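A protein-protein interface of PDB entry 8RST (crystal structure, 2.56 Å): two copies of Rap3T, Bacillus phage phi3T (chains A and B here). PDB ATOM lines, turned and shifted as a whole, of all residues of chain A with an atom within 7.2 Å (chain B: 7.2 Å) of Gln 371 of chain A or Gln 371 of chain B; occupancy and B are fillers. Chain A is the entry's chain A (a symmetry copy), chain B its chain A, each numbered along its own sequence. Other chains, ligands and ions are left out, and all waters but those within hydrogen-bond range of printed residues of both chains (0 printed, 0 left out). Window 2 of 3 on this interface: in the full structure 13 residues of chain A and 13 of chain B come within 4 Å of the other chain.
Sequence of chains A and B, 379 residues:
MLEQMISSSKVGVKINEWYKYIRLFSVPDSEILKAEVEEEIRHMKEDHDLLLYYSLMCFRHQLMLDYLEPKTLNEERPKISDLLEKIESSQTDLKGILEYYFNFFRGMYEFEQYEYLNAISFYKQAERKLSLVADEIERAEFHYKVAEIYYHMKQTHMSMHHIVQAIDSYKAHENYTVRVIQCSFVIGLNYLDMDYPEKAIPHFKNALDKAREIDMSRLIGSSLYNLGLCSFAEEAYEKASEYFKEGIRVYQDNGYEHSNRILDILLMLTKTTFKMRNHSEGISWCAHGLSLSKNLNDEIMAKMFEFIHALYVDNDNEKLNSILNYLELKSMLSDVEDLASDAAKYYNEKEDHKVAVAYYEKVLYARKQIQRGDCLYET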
ATOM      1  N   MET A 153     -22.671  19.400  14.725  1.00  0.00           N
ATOM      2  CA  MET A 153     -24.068  19.760  14.533  1.00  0.00           C
ATOM      3  C   MET A 153     -24.491  19.673  13.074  1.00  0.00           C
ATOM      4  O   MET A 153     -25.647  19.977  12.759  1.00  0.00           O
ATOM      5  CB  MET A 153     -24.335  21.172  15.066  1.00  0.00           C
ATOM      6  CG  MET A 153     -24.072  21.372  16.563  1.00  0.00           C
ATOM      7  SD  MET A 153     -25.206  20.474  17.640  1.00  0.00           S
ATOM      8  CE  MET A 153     -24.310  18.947  17.913  1.00  0.00           C
ATOM      9  N   LYS A 154     -23.583  19.263  12.184  1.00  0.00           N
ATOM     10  CA  LYS A 154     -23.832  19.203  10.742  1.00  0.00           C
ATOM     11  C   LYS A 154     -24.305  20.551  10.206  1.00  0.00           C
ATOM     12  O   LYS A 154     -25.110  20.627   9.275  1.00  0.00           O
ATOM     13  CB  LYS A 154     -24.821  18.087  10.397  1.00  0.00           C
ATOM     14  CG  LYS A 154     -24.662  17.545   8.982  1.00  0.00           C
ATOM     15  CD  LYS A 154     -25.109  16.096   8.895  1.00  0.00           C
ATOM     16  CE  LYS A 154     -25.000  15.561   7.477  1.00  0.00           C
ATOM     17  NZ  LYS A 154     -25.915  16.288   6.555  1.00  0.00           N
ATOM     18  N   GLN A 155     -23.805  21.631  10.808  1.00  0.00           N
ATOM     19  CA  GLN A 155     -24.002  22.985  10.291  1.00  0.00           C
ATOM     20  C   GLN A 155     -22.821  23.288   9.373  1.00  0.00           C
ATOM     21  O   GLN A 155     -21.857  23.966   9.737  1.00  0.00           O
ATOM     22  CB  GLN A 155     -24.123  23.987  11.433  1.00  0.00           C
ATOM     23  CG  GLN A 155     -25.260  23.694  12.405  1.00  0.00           C
ATOM     24  CD  GLN A 155     -26.627  23.814  11.759  1.00  0.00           C
ATOM     25  OE1 GLN A 155     -27.037  24.899  11.347  1.00  0.00           O
ATOM     26  NE2 GLN A 155     -27.340  22.697  11.668  1.00  0.00           N
ATOM     27  N   THR A 156     -22.910  22.762   8.149  1.00  0.00           N
ATOM     28  CA  THR A 156     -21.743  22.694   7.273  1.00  0.00           C
ATOM     29  C   THR A 156     -21.278  24.078   6.836  1.00  0.00           C
ATOM     30  O   THR A 156     -20.073  24.359   6.833  1.00  0.00           O
ATOM     31  CB  THR A 156     -22.058  21.833   6.051  1.00  0.00           C
ATOM     32  OG1 THR A 156     -22.684  20.615   6.475  1.00  0.00           O
ATOM     33  CG2 THR A 156     -20.783  21.500   5.295  1.00  0.00           C
ATOM     34  N   HIS A 157     -22.214  24.950   6.456  1.00  0.00           N
ATOM     35  CA  HIS A 157     -21.836  26.275   5.974  1.00  0.00           C
ATOM     36  C   HIS A 157     -21.158  27.090   7.069  1.00  0.00           C
ATOM     37  O   HIS A 157     -20.175  27.795   6.811  1.00  0.00           O
ATOM     38  CB  HIS A 157     -23.066  27.009   5.440  1.00  0.00           C
ATOM     39  CG  HIS A 157     -23.698  26.345   4.255  1.00  0.00           C
ATOM     40  ND1 HIS A 157     -22.994  26.035   3.112  1.00  0.00           N
ATOM     41  CD2 HIS A 157     -24.971  25.939   4.034  1.00  0.00           C
ATOM     42  CE1 HIS A 157     -23.803  25.462   2.239  1.00  0.00           C
ATOM     43  NE2 HIS A 157     -25.009  25.392   2.774  1.00  0.00           N
ATOM     44  N   ASP A 193     -19.650  15.564   4.367  1.00  0.00           N
ATOM     45  CA  ASP A 193     -21.067  15.780   4.638  1.00  0.00           C
ATOM     46  C   ASP A 193     -21.793  16.331   3.419  1.00  0.00           C
ATOM     47  O   ASP A 193     -23.004  16.129   3.275  1.00  0.00           O
ATOM     48  CB  ASP A 193     -21.244  16.719   5.833  1.00  0.00           C
ATOM     49  CG  ASP A 193     -21.054  16.013   7.161  1.00  0.00           C
ATOM     50  OD1 ASP A 193     -21.124  14.767   7.187  1.00  0.00           O
ATOM     51  OD2 ASP A 193     -20.849  16.702   8.182  1.00  0.00           O
ATOM     52  N   MET A 194     -21.077  17.026   2.536  1.00  0.00           N
ATOM     53  CA  MET A 194     -21.639  17.506   1.284  1.00  0.00           C
ATOM     54  C   MET A 194     -21.538  16.475   0.167  1.00  0.00           C
ATOM     55  O   MET A 194     -21.701  16.829  -1.006  1.00  0.00           O
ATOM     56  CB  MET A 194     -20.954  18.806   0.858  1.00  0.00           C
ATOM     57  CG  MET A 194     -21.090  19.947   1.851  1.00  0.00           C
ATOM     58  SD  MET A 194     -20.555  21.520   1.151  1.00  0.00           S
ATOM     59  CE  MET A 194     -18.981  21.047   0.444  1.00  0.00           C
ATOM     60  N   LEU A 333     -28.436  15.291  15.988  1.00  0.00           N
ATOM     61  CA  LEU A 333     -29.314  14.978  14.865  1.00  0.00           C
ATOM     62  C   LEU A 333     -28.563  14.312  13.719  1.00  0.00           C
ATOM     63  O   LEU A 333     -29.169  13.584  12.925  1.00  0.00           O
ATOM     64  CB  LEU A 333     -30.004  16.252  14.376  1.00  0.00           C
ATOM     65  CG  LEU A 333     -31.035  16.869  15.322  1.00  0.00           C
ATOM     66  CD1 LEU A 333     -31.329  18.312  14.943  1.00  0.00           C
ATOM     67  CD2 LEU A 333     -32.313  16.045  15.321  1.00  0.00           C
ATOM     68  N   TYR A 365     -36.894  13.780   8.462  1.00  0.00           N
ATOM     69  CA  TYR A 365     -37.179  14.603   9.632  1.00  0.00           C
ATOM     70  C   TYR A 365     -35.898  15.174  10.226  1.00  0.00           C
ATOM     71  O   TYR A 365     -35.830  16.363  10.557  1.00  0.00           O
ATOM     72  CB  TYR A 365     -37.940  13.781  10.674  1.00  0.00           C
ATOM     73  CG  TYR A 365     -38.121  14.485  12.001  1.00  0.00           C
ATOM     74  CD1 TYR A 365     -39.178  15.363  12.204  1.00  0.00           C
ATOM     75  CD2 TYR A 365     -37.237  14.269  13.050  1.00  0.00           C
ATOM     76  CE1 TYR A 365     -39.345  16.008  13.415  1.00  0.00           C
ATOM     77  CE2 TYR A 365     -37.397  14.910  14.263  1.00  0.00           C
ATOM     78  CZ  TYR A 365     -38.453  15.778  14.440  1.00  0.00           C
ATOM     79  OH  TYR A 365     -38.617  16.418  15.647  1.00  0.00           O
ATOM     80  N   ALA A 366     -34.867  14.337  10.367  1.00  0.00           N
ATOM     81  CA  ALA A 366     -33.618  14.804  10.959  1.00  0.00           C
ATOM     82  C   ALA A 366     -32.947  15.852  10.080  1.00  0.00           C
ATOM     83  O   ALA A 366     -32.392  16.832  10.589  1.00  0.00           O
ATOM     84  CB  ALA A 366     -32.677  13.625  11.208  1.00  0.00           C
ATOM     85  N   ARG A 367     -32.995  15.669   8.758  1.00  0.00           N
ATOM     86  CA  ARG A 367     -32.377  16.638   7.859  1.00  0.00           C
ATOM     87  C   ARG A 367     -33.066  17.994   7.946  1.00  0.00           C
ATOM     88  O   ARG A 367     -32.406  19.039   7.893  1.00  0.00           O
ATOM     89  CB  ARG A 367     -32.399  16.118   6.423  1.00  0.00           C
ATOM     90  CG  ARG A 367     -31.353  15.060   6.147  1.00  0.00           C
ATOM     91  CD  ARG A 367     -31.098  14.902   4.659  1.00  0.00           C
ATOM     92  NE  ARG A 367     -29.705  14.568   4.387  1.00  0.00           N
ATOM     93  CZ  ARG A 367     -28.831  15.390   3.821  1.00  0.00           C
ATOM     94  NH1 ARG A 367     -29.186  16.592   3.399  1.00  0.00           N
ATOM     95  NH2 ARG A 367     -27.571  14.993   3.672  1.00  0.00           N
ATOM     96  N   LYS A 368     -34.394  17.999   8.074  1.00  0.00           N
ATOM     97  CA  LYS A 368     -35.113  19.259   8.222  1.00  0.00           C
ATOM     98  C   LYS A 368     -34.764  19.936   9.541  1.00  0.00           C
ATOM     99  O   LYS A 368     -34.611  21.162   9.595  1.00  0.00           O
ATOM    100  CB  LYS A 368     -36.619  19.019   8.117  1.00  0.00           C
ATOM    101  N   GLN A 369     -34.633  19.152  10.616  1.00  0.00           N
ATOM    102  CA  GLN A 369     -34.239  19.715  11.905  1.00  0.00           C
ATOM    103  C   GLN A 369     -32.827  20.279  11.848  1.00  0.00           C
ATOM    104  O   GLN A 369     -32.554  21.354  12.397  1.00  0.00           O
ATOM    105  CB  GLN A 369     -34.341  18.650  12.997  1.00  0.00           C
ATOM    106  CG  GLN A 369     -35.752  18.193  13.310  1.00  0.00           C
ATOM    107  CD  GLN A 369     -36.595  19.290  13.922  1.00  0.00           C
ATOM    108  OE1 GLN A 369     -37.611  19.695  13.359  1.00  0.00           O
ATOM    109  NE2 GLN A 369     -36.179  19.777  15.085  1.00  0.00           N
ATOM    110  N   ILE A 370     -31.910  19.557  11.200  1.00  0.00           N
ATOM    111  CA  ILE A 370     -30.562  20.073  10.981  1.00  0.00           C
ATOM    112  C   ILE A 370     -30.620  21.377  10.197  1.00  0.00           C
ATOM    113  O   ILE A 370     -29.876  22.326  10.477  1.00  0.00           O
ATOM    114  CB  ILE A 370     -29.701  19.019  10.260  1.00  0.00           C
ATOM    115  CG1 ILE A 370     -29.456  17.809  11.163  1.00  0.00           C
ATOM    116  CG2 ILE A 370     -28.381  19.618   9.799  1.00  0.00           C
ATOM    117  CD1 ILE A 370     -28.806  16.642  10.454  1.00  0.00           C
ATOM    118  N   GLN A 371     -31.518  21.449   9.211  1.00  0.00           N
ATOM    119  CA  GLN A 371     -31.609  22.640   8.377  1.00  0.00           C
ATOM    120  C   GLN A 371     -32.148  23.837   9.152  1.00  0.00           C
ATOM    121  O   GLN A 371     -31.859  24.982   8.790  1.00  0.00           O
ATOM    122  CB  GLN A 371     -32.488  22.360   7.158  1.00  0.00           C
ATOM    123  CG  GLN A 371     -32.121  23.171   5.927  1.00  0.00           C
ATOM    124  CD  GLN A 371     -30.933  22.590   5.187  1.00  0.00           C
ATOM    125  OE1 GLN A 371     -30.323  21.618   5.634  1.00  0.00           O
ATOM    126  NE2 GLN A 371     -30.605  23.176   4.043  1.00  0.00           N
ATOM    127  N   ARG A 372     -32.918  23.595  10.216  1.00  0.00           N
ATOM    128  CA  ARG A 372     -33.545  24.691  10.949  1.00  0.00           C
ATOM    129  C   ARG A 372     -32.509  25.575  11.639  1.00  0.00           C
ATOM    130  O   ARG A 372     -32.703  26.793  11.754  1.00  0.00           O
ATOM    131  CB  ARG A 372     -34.541  24.132  11.965  1.00  0.00           C
ATOM    132  CG  ARG A 372     -35.967  24.001  11.427  1.00  0.00           C
ATOM    133  CD  ARG A 372     -36.747  22.890  12.116  1.00  0.00           C
ATOM    134  NE  ARG A 372     -38.175  22.966  11.826  1.00  0.00           N
ATOM    135  CZ  ARG A 372     -39.092  23.394  12.684  1.00  0.00           C
ATOM    136  NH1 ARG A 372     -38.770  23.754  13.917  1.00  0.00           N
ATOM    137  NH2 ARG A 372     -40.362  23.462  12.297  1.00  0.00           N
ATOM    138  N   GLY A 373     -31.409  24.981  12.107  1.00  0.00           N
ATOM    139  CA  GLY A 373     -30.348  25.737  12.751  1.00  0.00           C
ATOM    140  C   GLY A 373     -30.769  26.487  13.999  1.00  0.00           C
ATOM    141  O   GLY A 373     -31.142  25.884  15.005  1.00  0.00           O
ATOM    142  N   ASP A 374     -30.703  27.810  13.948  1.00  0.00           N
ATOM    143  CA  ASP A 374     -31.074  28.663  15.071  1.00  0.00           C
ATOM    144  C   ASP A 374     -32.534  29.096  14.964  1.00  0.00           C
ATOM    145  O   ASP A 374     -33.441  28.301  15.203  1.00  0.00           O
ATOM    146  CB  ASP A 374     -30.162  29.889  15.121  1.00  0.00           C
ATOM    147  N   MET B 153     -33.985  28.707  -5.764  1.00  0.00           N
ATOM    148  CA  MET B 153     -33.001  27.640  -5.667  1.00  0.00           C
ATOM    149  C   MET B 153     -33.030  26.950  -4.309  1.00  0.00           C
ATOM    150  O   MET B 153     -32.228  26.041  -4.075  1.00  0.00           O
ATOM    151  CB  MET B 153     -31.593  28.182  -5.941  1.00  0.00           C
ATOM    152  CG  MET B 153     -31.382  28.794  -7.330  1.00  0.00           C
ATOM    153  SD  MET B 153     -31.467  27.605  -8.684  1.00  0.00           S
ATOM    154  CE  MET B 153     -33.194  27.706  -9.146  1.00  0.00           C
ATOM    155  N   LYS B 154     -33.937  27.364  -3.420  1.00  0.00           N
ATOM    156  CA  LYS B 154     -34.027  26.841  -2.055  1.00  0.00           C
ATOM    157  C   LYS B 154     -32.693  26.968  -1.323  1.00  0.00           C
ATOM    158  O   LYS B 154     -32.333  26.131  -0.494  1.00  0.00           O
ATOM    159  CB  LYS B 154     -34.532  25.396  -2.047  1.00  0.00           C
ATOM    160  CG  LYS B 154     -35.237  25.000  -0.756  1.00  0.00           C
ATOM    161  CD  LYS B 154     -36.269  23.914  -1.005  1.00  0.00           C
ATOM    162  CE  LYS B 154     -36.945  23.479   0.285  1.00  0.00           C
ATOM    163  NZ  LYS B 154     -35.968  22.856   1.221  1.00  0.00           N
ATOM    164  N   GLN B 155     -31.947  28.025  -1.643  1.00  0.00           N
ATOM    165  CA  GLN B 155     -30.744  28.396  -0.898  1.00  0.00           C
ATOM    166  C   GLN B 155     -31.177  29.376   0.189  1.00  0.00           C
ATOM    167  O   GLN B 155     -31.033  30.595   0.076  1.00  0.00           O
ATOM    168  CB  GLN B 155     -29.692  28.988  -1.829  1.00  0.00           C
ATOM    169  CG  GLN B 155     -29.267  28.063  -2.961  1.00  0.00           C
ATOM    170  CD  GLN B 155     -28.555  26.819  -2.466  1.00  0.00           C
ATOM    171  OE1 GLN B 155     -27.465  26.899  -1.898  1.00  0.00           O
ATOM    172  NE2 GLN B 155     -29.170  25.660  -2.675  1.00  0.00           N
ATOM    173  N   THR B 156     -31.724  28.812   1.269  1.00  0.00           N
ATOM    174  CA  THR B 156     -32.463  29.612   2.242  1.00  0.00           C
ATOM    175  C   THR B 156     -31.556  30.582   2.989  1.00  0.00           C
ATOM    176  O   THR B 156     -31.916  31.749   3.184  1.00  0.00           O
ATOM    177  CB  THR B 156     -33.185  28.696   3.229  1.00  0.00           C
ATOM    178  OG1 THR B 156     -33.871  27.664   2.508  1.00  0.00           O
ATOM    179  CG2 THR B 156     -34.193  29.487   4.047  1.00  0.00           C
ATOM    180  N   HIS B 157     -30.383  30.116   3.424  1.00  0.00           N
ATOM    181  CA  HIS B 157     -29.488  30.973   4.194  1.00  0.00           C
ATOM    182  C   HIS B 157     -29.002  32.155   3.363  1.00  0.00           C
ATOM    183  O   HIS B 157     -28.916  33.283   3.864  1.00  0.00           O
ATOM    184  CB  HIS B 157     -28.304  30.160   4.719  1.00  0.00           C
ATOM    185  CG  HIS B 157     -28.694  29.072   5.671  1.00  0.00           C
ATOM    186  ND1 HIS B 157     -29.442  29.308   6.805  1.00  0.00           N
ATOM    187  CD2 HIS B 157     -28.433  27.743   5.663  1.00  0.00           C
ATOM    188  CE1 HIS B 157     -29.630  28.172   7.451  1.00  0.00           C
ATOM    189  NE2 HIS B 157     -29.027  27.206   6.780  1.00  0.00           N
ATOM    190  N   ASP B 193     -39.963  27.471   3.923  1.00  0.00           N
ATOM    191  CA  ASP B 193     -39.041  26.408   3.540  1.00  0.00           C
ATOM    192  C   ASP B 193     -38.343  25.809   4.752  1.00  0.00           C
ATOM    193  O   ASP B 193     -37.929  24.644   4.716  1.00  0.00           O
ATOM    194  CB  ASP B 193     -38.010  26.933   2.539  1.00  0.00           C
ATOM    195  CG  ASP B 193     -38.561  27.021   1.128  1.00  0.00           C
ATOM    196  OD1 ASP B 193     -39.593  26.377   0.853  1.00  0.00           O
ATOM    197  OD2 ASP B 193     -37.954  27.722   0.292  1.00  0.00           O
ATOM    198  N   MET B 194     -38.204  26.580   5.829  1.00  0.00           N
ATOM    199  CA  MET B 194     -37.653  26.081   7.080  1.00  0.00           C
ATOM    200  C   MET B 194     -38.716  25.462   7.977  1.00  0.00           C
ATOM    201  O   MET B 194     -38.464  25.261   9.171  1.00  0.00           O
ATOM    202  CB  MET B 194     -36.927  27.201   7.826  1.00  0.00           C
ATOM    203  CG  MET B 194     -35.765  27.818   7.063  1.00  0.00           C
ATOM    204  SD  MET B 194     -34.760  28.885   8.113  1.00  0.00           S
ATOM    205  CE  MET B 194     -36.032  29.876   8.889  1.00  0.00           C
ATOM    206  N   LEU B 333     -34.497  22.055  -8.450  1.00  0.00           N
ATOM    207  CA  LEU B 333     -34.454  20.935  -7.517  1.00  0.00           C
ATOM    208  C   LEU B 333     -35.532  21.041  -6.444  1.00  0.00           C
ATOM    209  O   LEU B 333     -35.944  20.021  -5.881  1.00  0.00           O
ATOM    210  CB  LEU B 333     -33.072  20.849  -6.871  1.00  0.00           C
ATOM    211  CG  LEU B 333     -31.919  20.439  -7.788  1.00  0.00           C
ATOM    212  CD1 LEU B 333     -30.576  20.795  -7.173  1.00  0.00           C
ATOM    213  CD2 LEU B 333     -31.990  18.951  -8.093  1.00  0.00           C
ATOM    214  N   TYR B 365     -32.430  12.608  -2.372  1.00  0.00           N
ATOM    215  CA  TYR B 365     -31.448  12.980  -3.384  1.00  0.00           C
ATOM    216  C   TYR B 365     -31.529  14.467  -3.705  1.00  0.00           C
ATOM    217  O   TYR B 365     -30.504  15.152  -3.790  1.00  0.00           O
ATOM    218  CB  TYR B 365     -31.657  12.141  -4.647  1.00  0.00           C
ATOM    219  CG  TYR B 365     -30.810  12.576  -5.822  1.00  0.00           C
ATOM    220  CD1 TYR B 365     -29.505  12.123  -5.970  1.00  0.00           C
ATOM    221  CD2 TYR B 365     -31.318  13.438  -6.787  1.00  0.00           C
ATOM    222  CE1 TYR B 365     -28.730  12.520  -7.042  1.00  0.00           C
ATOM    223  CE2 TYR B 365     -30.549  13.840  -7.861  1.00  0.00           C
ATOM    224  CZ  TYR B 365     -29.257  13.377  -7.985  1.00  0.00           C
ATOM    225  OH  TYR B 365     -28.487  13.775  -9.054  1.00  0.00           O
ATOM    226  N   ALA B 366     -32.746  14.984  -3.890  1.00  0.00           N
ATOM    227  CA  ALA B 366     -32.901  16.393  -4.233  1.00  0.00           C
ATOM    228  C   ALA B 366     -32.435  17.295  -3.097  1.00  0.00           C
ATOM    229  O   ALA B 366     -31.812  18.334  -3.339  1.00  0.00           O
ATOM    230  CB  ALA B 366     -34.355  16.692  -4.598  1.00  0.00           C
ATOM    231  N   ARG B 367     -32.718  16.910  -1.850  1.00  0.00           N
ATOM    232  CA  ARG B 367     -32.295  17.724  -0.715  1.00  0.00           C
ATOM    233  C   ARG B 367     -30.777  17.790  -0.614  1.00  0.00           C
ATOM    234  O   ARG B 367     -30.215  18.841  -0.285  1.00  0.00           O
ATOM    235  CB  ARG B 367     -32.895  17.179   0.580  1.00  0.00           C
ATOM    236  CG  ARG B 367     -34.357  17.524   0.762  1.00  0.00           C
ATOM    237  CD  ARG B 367     -34.788  17.378   2.209  1.00  0.00           C
ATOM    238  NE  ARG B 367     -35.801  18.365   2.568  1.00  0.00           N
ATOM    239  CZ  ARG B 367     -35.595  19.395   3.378  1.00  0.00           C
ATOM    240  NH1 ARG B 367     -34.433  19.576   3.983  1.00  0.00           N
ATOM    241  NH2 ARG B 367     -36.582  20.260   3.590  1.00  0.00           N
ATOM    242  N   LYS B 368     -30.096  16.676  -0.888  1.00  0.00           N
ATOM    243  CA  LYS B 368     -28.638  16.684  -0.869  1.00  0.00           C
ATOM    244  C   LYS B 368     -28.080  17.561  -1.984  1.00  0.00           C
ATOM    245  O   LYS B 368     -27.097  18.283  -1.779  1.00  0.00           O
ATOM    246  CB  LYS B 368     -28.104  15.256  -0.984  1.00  0.00           C
ATOM    247  N   GLN B 369     -28.697  17.512  -3.168  1.00  0.00           N
ATOM    248  CA  GLN B 369     -28.264  18.367  -4.269  1.00  0.00           C
ATOM    249  C   GLN B 369     -28.490  19.837  -3.943  1.00  0.00           C
ATOM    250  O   GLN B 369     -27.640  20.686  -4.239  1.00  0.00           O
ATOM    251  CB  GLN B 369     -29.004  17.989  -5.552  1.00  0.00           C
ATOM    252  CG  GLN B 369     -28.658  16.621  -6.107  1.00  0.00           C
ATOM    253  CD  GLN B 369     -27.225  16.535  -6.585  1.00  0.00           C
ATOM    254  OE1 GLN B 369     -26.434  15.744  -6.073  1.00  0.00           O
ATOM    255  NE2 GLN B 369     -26.881  17.349  -7.576  1.00  0.00           N
ATOM    256  N   ILE B 370     -29.641  20.156  -3.350  1.00  0.00           N
ATOM    257  CA  ILE B 370     -29.895  21.516  -2.882  1.00  0.00           C
ATOM    258  C   ILE B 370     -28.835  21.930  -1.871  1.00  0.00           C
ATOM    259  O   ILE B 370     -28.359  23.074  -1.874  1.00  0.00           O
ATOM    260  CB  ILE B 370     -31.313  21.617  -2.287  1.00  0.00           C
ATOM    261  CG1 ILE B 370     -32.371  21.431  -3.375  1.00  0.00           C
ATOM    262  CG2 ILE B 370     -31.508  22.946  -1.572  1.00  0.00           C
ATOM    263  CD1 ILE B 370     -33.779  21.299  -2.838  1.00  0.00           C
ATOM    264  N   GLN B 371     -28.437  21.002  -0.999  1.00  0.00           N
ATOM    265  CA  GLN B 371     -27.463  21.324   0.036  1.00  0.00           C
ATOM    266  C   GLN B 371     -26.078  21.578  -0.548  1.00  0.00           C
ATOM    267  O   GLN B 371     -25.279  22.297   0.061  1.00  0.00           O
ATOM    268  CB  GLN B 371     -27.404  20.199   1.068  1.00  0.00           C
ATOM    269  CG  GLN B 371     -27.030  20.658   2.468  1.00  0.00           C
ATOM    270  CD  GLN B 371     -28.206  21.260   3.210  1.00  0.00           C
ATOM    271  OE1 GLN B 371     -29.294  21.411   2.656  1.00  0.00           O
ATOM    272  NE2 GLN B 371     -27.996  21.597   4.476  1.00  0.00           N
ATOM    273  N   ARG B 372     -25.781  21.010  -1.719  1.00  0.00           N
ATOM    274  CA  ARG B 372     -24.443  21.132  -2.291  1.00  0.00           C
ATOM    275  C   ARG B 372     -24.122  22.574  -2.673  1.00  0.00           C
ATOM    276  O   ARG B 372     -22.965  23.006  -2.569  1.00  0.00           O
ATOM    277  CB  ARG B 372     -24.311  20.210  -3.502  1.00  0.00           C
ATOM    278  CG  ARG B 372     -23.774  18.817  -3.165  1.00  0.00           C
ATOM    279  CD  ARG B 372     -24.260  17.756  -4.142  1.00  0.00           C
ATOM    280  NE  ARG B 372     -23.516  16.509  -4.007  1.00  0.00           N
ATOM    281  CZ  ARG B 372     -22.593  16.090  -4.863  1.00  0.00           C
ATOM    282  NH1 ARG B 372     -22.305  16.776  -5.957  1.00  0.00           N
ATOM    283  NH2 ARG B 372     -21.945  14.955  -4.617  1.00  0.00           N
ATOM    284  N   GLY B 373     -25.128  23.330  -3.120  1.00  0.00           N
ATOM    285  CA  GLY B 373     -24.935  24.725  -3.480  1.00  0.00           C
ATOM    286  C   GLY B 373     -23.938  24.961  -4.598  1.00  0.00           C
ATOM    287  O   GLY B 373     -24.156  24.551  -5.737  1.00  0.00           O
ATOM    288  N   ASP B 374     -22.840  25.633  -4.282  1.00  0.00           N
ATOM    289  CA  ASP B 374     -21.795  25.937  -5.253  1.00  0.00           C
ATOM    290  C   ASP B 374     -20.706  24.866  -5.229  1.00  0.00           C
ATOM    291  O   ASP B 374     -20.910  23.758  -5.720  1.00  0.00           O
ATOM    292  CB  ASP B 374     -21.191  27.310  -4.960  1.00  0.00           C
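The side-chain amide oxygen of Gln 371 of chain B sits at hydrogen-bond distance from the side-chain amide nitrogen of Gln 371 of chain A, at 2.6 Å.
Among the printed residues, pairs that only touch across the chains: Arg 372 of chain A with Met 194 of chain B (3.5 Å) and Met 194 of chain A with Arg 372 of chain B (3.5 Å).
Gln 371 of chain B touches one residue of chain A. Of the printed residues of chain B, Met 194 of chain A touches Arg 372 (3.5 Å). Printed residues of chain A within 4 Å of Met 194 of chain B: Arg 372. Of the printed residues of chain A, Arg 372 of chain B touches Met 194 (3.5 Å). Arg 367 of chain B touches none of the printed residues of chain A. Lys 368 of chain A touches none of the printed residues of chain B. The nearest residue of chain A that does not touch Gln 371 of chain B is His 157 of chain A (4.1 Å). The nearest printed residue of chain B that does not touch Arg 372 of chain A is His 157 of chain B (5.5 Å).
Among the printed residues, no Asp or Glu carboxylate lies within 4 Å of a Lys or Arg side-chain nitrogen of the other chain.
Met 194 of chain A touches Arg 372 of chain B, and with the chains exchanged Arg 372 of chain A touches Met 194 of chain B. Gln 371 of chain B touches its own counterpart, Gln 371 of chain A. 18 positions are printed for both chains. Of the 3 pairs that touch across the chains among the printed residues, 3 have their exchanged pair printed and touching as well.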
